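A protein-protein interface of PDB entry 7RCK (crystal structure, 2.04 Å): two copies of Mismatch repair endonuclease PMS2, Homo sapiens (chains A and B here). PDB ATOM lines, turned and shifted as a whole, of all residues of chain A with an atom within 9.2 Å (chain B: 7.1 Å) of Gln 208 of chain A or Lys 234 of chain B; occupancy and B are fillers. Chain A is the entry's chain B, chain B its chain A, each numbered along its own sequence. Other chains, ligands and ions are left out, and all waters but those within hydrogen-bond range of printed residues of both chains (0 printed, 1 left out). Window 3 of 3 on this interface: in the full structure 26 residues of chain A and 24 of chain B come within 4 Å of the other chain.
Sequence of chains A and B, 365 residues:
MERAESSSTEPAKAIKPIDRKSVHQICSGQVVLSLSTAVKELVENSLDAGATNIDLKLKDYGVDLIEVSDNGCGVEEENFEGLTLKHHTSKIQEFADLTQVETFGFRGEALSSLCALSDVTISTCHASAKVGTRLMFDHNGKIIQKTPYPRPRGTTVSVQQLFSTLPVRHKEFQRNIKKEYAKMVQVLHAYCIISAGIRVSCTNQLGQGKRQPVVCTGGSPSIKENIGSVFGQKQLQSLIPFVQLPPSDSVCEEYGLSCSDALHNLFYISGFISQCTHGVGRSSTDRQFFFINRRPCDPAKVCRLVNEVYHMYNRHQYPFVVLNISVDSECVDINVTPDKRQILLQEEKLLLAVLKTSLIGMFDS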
ATOM      1  N   LYS A  59      -6.839  10.897   4.009  1.00  0.00           N
ATOM      2  CA  LYS A  59      -7.753  11.442   3.016  1.00  0.00           C
ATOM      3  C   LYS A  59      -7.688  10.550   1.787  1.00  0.00           C
ATOM      4  O   LYS A  59      -6.600  10.303   1.256  1.00  0.00           O
ATOM      5  CB  LYS A  59      -7.398  12.888   2.654  1.00  0.00           C
ATOM      6  CG  LYS A  59      -7.642  13.888   3.774  1.00  0.00           C
ATOM      7  N   ASP A  60      -8.852  10.069   1.344  1.00  0.00           N
ATOM      8  CA  ASP A  60      -8.945   9.138   0.218  1.00  0.00           C
ATOM      9  C   ASP A  60      -8.082   7.900   0.463  1.00  0.00           C
ATOM     10  O   ASP A  60      -7.301   7.478  -0.393  1.00  0.00           O
ATOM     11  CB  ASP A  60      -8.570   9.824  -1.099  1.00  0.00           C
ATOM     12  CG  ASP A  60      -9.604  10.843  -1.543  1.00  0.00           C
ATOM     13  OD1 ASP A  60     -10.691  10.898  -0.931  1.00  0.00           O
ATOM     14  OD2 ASP A  60      -9.328  11.594  -2.502  1.00  0.00           O
ATOM     15  N   GLN A 205     -11.280  10.354   5.380  1.00  0.00           N
ATOM     16  CA  GLN A 205     -12.225  11.257   4.732  1.00  0.00           C
ATOM     17  C   GLN A 205     -12.160  11.005   3.233  1.00  0.00           C
ATOM     18  O   GLN A 205     -11.082  11.078   2.637  1.00  0.00           O
ATOM     19  CB  GLN A 205     -11.909  12.718   5.072  1.00  0.00           C
ATOM     20  CG  GLN A 205     -12.938  13.720   4.578  1.00  0.00           C
ATOM     21  CD  GLN A 205     -12.571  15.148   4.939  1.00  0.00           C
ATOM     22  OE1 GLN A 205     -11.393  15.501   5.016  1.00  0.00           O
ATOM     23  NE2 GLN A 205     -13.582  15.974   5.183  1.00  0.00           N
ATOM     24  N   LEU A 206     -13.310  10.710   2.626  1.00  0.00           N
ATOM     25  CA  LEU A 206     -13.397  10.332   1.217  1.00  0.00           C
ATOM     26  C   LEU A 206     -13.987  11.467   0.389  1.00  0.00           C
ATOM     27  O   LEU A 206     -15.162  11.815   0.557  1.00  0.00           O
ATOM     28  CB  LEU A 206     -14.234   9.065   1.053  1.00  0.00           C
ATOM     29  CG  LEU A 206     -13.772   7.862   1.873  1.00  0.00           C
ATOM     30  CD1 LEU A 206     -14.655   6.654   1.597  1.00  0.00           C
ATOM     31  CD2 LEU A 206     -12.321   7.555   1.557  1.00  0.00           C
ATOM     32  N   GLY A 207     -13.180  12.028  -0.509  1.00  0.00           N
ATOM     33  CA  GLY A 207     -13.688  13.046  -1.415  1.00  0.00           C
ATOM     34  C   GLY A 207     -14.196  14.267  -0.674  1.00  0.00           C
ATOM     35  O   GLY A 207     -13.493  14.867   0.146  1.00  0.00           O
ATOM     36  N   GLN A 208     -15.438  14.643  -0.970  1.00  0.00           N
ATOM     37  CA  GLN A 208     -16.087  15.788  -0.351  1.00  0.00           C
ATOM     38  C   GLN A 208     -16.911  15.408   0.872  1.00  0.00           C
ATOM     39  O   GLN A 208     -17.623  16.259   1.413  1.00  0.00           O
ATOM     40  CB  GLN A 208     -16.992  16.491  -1.368  1.00  0.00           C
ATOM     41  CG  GLN A 208     -16.301  16.907  -2.655  1.00  0.00           C
ATOM     42  CD  GLN A 208     -15.574  18.229  -2.527  1.00  0.00           C
ATOM     43  OE1 GLN A 208     -14.453  18.290  -2.023  1.00  0.00           O
ATOM     44  NE2 GLN A 208     -16.214  19.302  -2.982  1.00  0.00           N
ATOM     45  N   GLY A 209     -16.830  14.156   1.319  1.00  0.00           N
ATOM     46  CA  GLY A 209     -17.620  13.698   2.440  1.00  0.00           C
ATOM     47  C   GLY A 209     -17.064  14.138   3.782  1.00  0.00           C
ATOM     48  O   GLY A 209     -16.024  14.787   3.891  1.00  0.00           O
ATOM     49  N   LYS A 210     -17.788  13.758   4.831  1.00  0.00           N
ATOM     50  CA  LYS A 210     -17.398  14.083   6.193  1.00  0.00           C
ATOM     51  C   LYS A 210     -16.265  13.175   6.656  1.00  0.00           C
ATOM     52  O   LYS A 210     -16.095  12.056   6.162  1.00  0.00           O
ATOM     53  CB  LYS A 210     -18.594  13.939   7.132  1.00  0.00           C
ATOM     54  CG  LYS A 210     -19.125  12.515   7.223  1.00  0.00           C
ATOM     55  CD  LYS A 210     -20.623  12.492   7.482  1.00  0.00           C
ATOM     56  CE  LYS A 210     -20.968  13.155   8.802  1.00  0.00           C
ATOM     57  NZ  LYS A 210     -20.305  12.482   9.952  1.00  0.00           N
ATOM     58  N   ARG A 211     -15.478  13.669   7.607  1.00  0.00           N
ATOM     59  CA  ARG A 211     -14.447  12.830   8.200  1.00  0.00           C
ATOM     60  C   ARG A 211     -15.093  11.756   9.067  1.00  0.00           C
ATOM     61  O   ARG A 211     -16.017  12.030   9.837  1.00  0.00           O
ATOM     62  CB  ARG A 211     -13.474  13.673   9.022  1.00  0.00           C
ATOM     63  CG  ARG A 211     -12.301  12.873   9.552  1.00  0.00           C
ATOM     64  CD  ARG A 211     -11.124  13.748   9.927  1.00  0.00           C
ATOM     65  NE  ARG A 211     -10.435  14.226   8.736  1.00  0.00           N
ATOM     66  CZ  ARG A 211      -9.718  13.456   7.927  1.00  0.00           C
ATOM     67  NH1 ARG A 211      -9.569  12.159   8.155  1.00  0.00           N
ATOM     68  NH2 ARG A 211      -9.141  13.998   6.859  1.00  0.00           N
ATOM     69  N   GLY B 228     -16.090  21.596   7.650  1.00  0.00           N
ATOM     70  CA  GLY B 228     -15.845  20.627   6.594  1.00  0.00           C
ATOM     71  C   GLY B 228     -15.709  19.210   7.119  1.00  0.00           C
ATOM     72  O   GLY B 228     -16.141  18.256   6.470  1.00  0.00           O
ATOM     73  N   PHE B 231     -19.598  18.170   8.269  1.00  0.00           N
ATOM     74  CA  PHE B 231     -20.630  18.066   7.250  1.00  0.00           C
ATOM     75  C   PHE B 231     -20.094  17.781   5.855  1.00  0.00           C
ATOM     76  O   PHE B 231     -20.895  17.549   4.943  1.00  0.00           O
ATOM     77  CB  PHE B 231     -21.471  19.352   7.214  1.00  0.00           C
ATOM     78  CG  PHE B 231     -22.157  19.664   8.515  1.00  0.00           C
ATOM     79  CD1 PHE B 231     -23.191  18.865   8.977  1.00  0.00           C
ATOM     80  CD2 PHE B 231     -21.777  20.762   9.271  1.00  0.00           C
ATOM     81  CE1 PHE B 231     -23.827  19.149  10.171  1.00  0.00           C
ATOM     82  CE2 PHE B 231     -22.410  21.052  10.468  1.00  0.00           C
ATOM     83  CZ  PHE B 231     -23.436  20.244  10.917  1.00  0.00           C
ATOM     84  N   GLY B 232     -18.783  17.786   5.660  1.00  0.00           N
ATOM     85  CA  GLY B 232     -18.212  17.563   4.351  1.00  0.00           C
ATOM     86  C   GLY B 232     -17.871  18.868   3.648  1.00  0.00           C
ATOM     87  O   GLY B 232     -18.382  19.943   3.974  1.00  0.00           O
ATOM     88  N   GLN B 233     -16.979  18.764   2.658  1.00  0.00           N
ATOM     89  CA  GLN B 233     -16.568  19.941   1.901  1.00  0.00           C
ATOM     90  C   GLN B 233     -17.697  20.503   1.050  1.00  0.00           C
ATOM     91  O   GLN B 233     -17.673  21.695   0.724  1.00  0.00           O
ATOM     92  CB  GLN B 233     -15.365  19.611   1.013  1.00  0.00           C
ATOM     93  CG  GLN B 233     -14.141  19.096   1.759  1.00  0.00           C
ATOM     94  CD  GLN B 233     -13.516  20.141   2.667  1.00  0.00           C
ATOM     95  OE1 GLN B 233     -14.012  20.412   3.760  1.00  0.00           O
ATOM     96  NE2 GLN B 233     -12.417  20.734   2.215  1.00  0.00           N
ATOM     97  N   LYS B 234     -18.679  19.675   0.680  1.00  0.00           N
ATOM     98  CA  LYS B 234     -19.802  20.170  -0.108  1.00  0.00           C
ATOM     99  C   LYS B 234     -20.600  21.219   0.656  1.00  0.00           C
ATOM    100  O   LYS B 234     -21.127  22.159   0.051  1.00  0.00           O
ATOM    101  CB  LYS B 234     -20.707  19.009  -0.521  1.00  0.00           C
ATOM    102  N   GLN B 235     -20.697  21.080   1.981  1.00  0.00           N
ATOM    103  CA  GLN B 235     -21.389  22.084   2.781  1.00  0.00           C
ATOM    104  C   GLN B 235     -20.665  23.425   2.745  1.00  0.00           C
ATOM    105  O   GLN B 235     -21.313  24.478   2.770  1.00  0.00           O
ATOM    106  CB  GLN B 235     -21.537  21.596   4.222  1.00  0.00           C
ATOM    107  CG  GLN B 235     -22.199  22.595   5.168  1.00  0.00           C
ATOM    108  CD  GLN B 235     -23.638  22.902   4.792  1.00  0.00           C
ATOM    109  OE1 GLN B 235     -24.564  22.228   5.238  1.00  0.00           O
ATOM    110  NE2 GLN B 235     -23.831  23.932   3.974  1.00  0.00           N
ATOM    111  N   LEU B 236     -19.331  23.410   2.676  1.00  0.00           N
ATOM    112  CA  LEU B 236     -18.562  24.649   2.644  1.00  0.00           C
ATOM    113  C   LEU B 236     -18.739  25.422   1.344  1.00  0.00           C
ATOM    114  O   LEU B 236     -18.540  26.642   1.334  1.00  0.00           O
ATOM    115  CB  LEU B 236     -17.076  24.355   2.859  1.00  0.00           C
ATOM    116  CG  LEU B 236     -16.626  23.983   4.272  1.00  0.00           C
ATOM    117  CD1 LEU B 236     -15.135  23.677   4.287  1.00  0.00           C
ATOM    118  CD2 LEU B 236     -16.952  25.108   5.242  1.00  0.00           C
ATOM    119  N   GLN B 237     -19.108  24.749   0.252  1.00  0.00           N
ATOM    120  CA  GLN B 237     -19.162  25.412  -1.046  1.00  0.00           C
ATOM    121  C   GLN B 237     -20.302  26.417  -1.150  1.00  0.00           C
ATOM    122  O   GLN B 237     -20.242  27.312  -2.000  1.00  0.00           O
ATOM    123  CB  GLN B 237     -19.288  24.373  -2.162  1.00  0.00           C
ATOM    124  CG  GLN B 237     -18.068  23.480  -2.322  1.00  0.00           C
ATOM    125  N   SER B 238     -21.330  26.300  -0.312  1.00  0.00           N
ATOM    126  CA  SER B 238     -22.473  27.203  -0.352  1.00  0.00           C
ATOM    127  C   SER B 238     -22.455  28.223   0.780  1.00  0.00           C
ATOM    128  O   SER B 238     -23.487  28.840   1.065  1.00  0.00           O
ATOM    129  CB  SER B 238     -23.776  26.404  -0.316  1.00  0.00           C
ATOM    130  OG  SER B 238     -23.922  25.730   0.920  1.00  0.00           O
ATOM    131  N   LEU B 239     -21.310  28.417   1.426  1.00  0.00           N
ATOM    132  CA  LEU B 239     -21.195  29.310   2.569  1.00  0.00           C
ATOM    133  C   LEU B 239     -20.358  30.533   2.216  1.00  0.00           C
ATOM    134  O   LEU B 239     -19.464  30.474   1.366  1.00  0.00           O
ATOM    135  CB  LEU B 239     -20.567  28.594   3.768  1.00  0.00           C
ATOM    136  CG  LEU B 239     -21.258  27.324   4.263  1.00  0.00           C
ATOM    137  CD1 LEU B 239     -20.608  26.827   5.544  1.00  0.00           C
ATOM    138  CD2 LEU B 239     -22.747  27.562   4.463  1.00  0.00           C
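O of Gln 208 of chain A is in hydrogen-bond range of N of Gln 233 of chain B (2.9 Å).
OE1 of Gln 205 of chain A lies within hydrogen-bond range of NH2 of Arg 211 of chain A, at 3.3 Å. The side-chain amide nitrogen (NE2) of Gln 205 of chain A lies within hydrogen-bond range of the backbone carbonyl oxygen (O) of Gly 209 of chain A (3.0 Å). N of Asp 60 of chain A lies within hydrogen-bond range of O of Gln 205 of chain A.
Among the printed residues, merely in contact across the chains: Gln 205 of chain A with Gly 228 of chain B, Gln 208 of chain A with Gly 232 of chain B, Gln 208 of chain A with Lys 234 of chain B, Gly 209 of chain A with Gly 232 of chain B and Lys 210 of chain A with Gly 232 of chain B.
Of chain B, only Gly 232, Gln 233 and Lys 234 come within 4 Å of Gln 208 of chain A. Lys 234 of chain B touches just one residue of chain A: Gln 208 (3.6 Å). Of the printed residues of chain B, Lys 210 of chain A touches Gly 232 (3.9 Å). Printed residues of chain A within 4 Å of Gln 233 of chain B: Gln 208 (2.9 Å). Printed residues of chain B within 4 Å of Gly 209 of chain A: Gly 232. Of the printed residues of chain A, Gly 228 of chain B touches Gln 205 (3.7 Å). The nearest residue of chain A that does not touch Lys 234 of chain B is Gly 209 of chain A (5.9 Å).
Of the 9 printed residues of chain A, 4 touch a printed residue of chain B. Of the 10 printed residues of chain B, 4 touch a printed residue of chain A. Among the printed residues, no Asp or Glu carboxylate lies within 4 Å of a Lys or Arg side-chain nitrogen of the other chain.
No position is printed for both chains.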
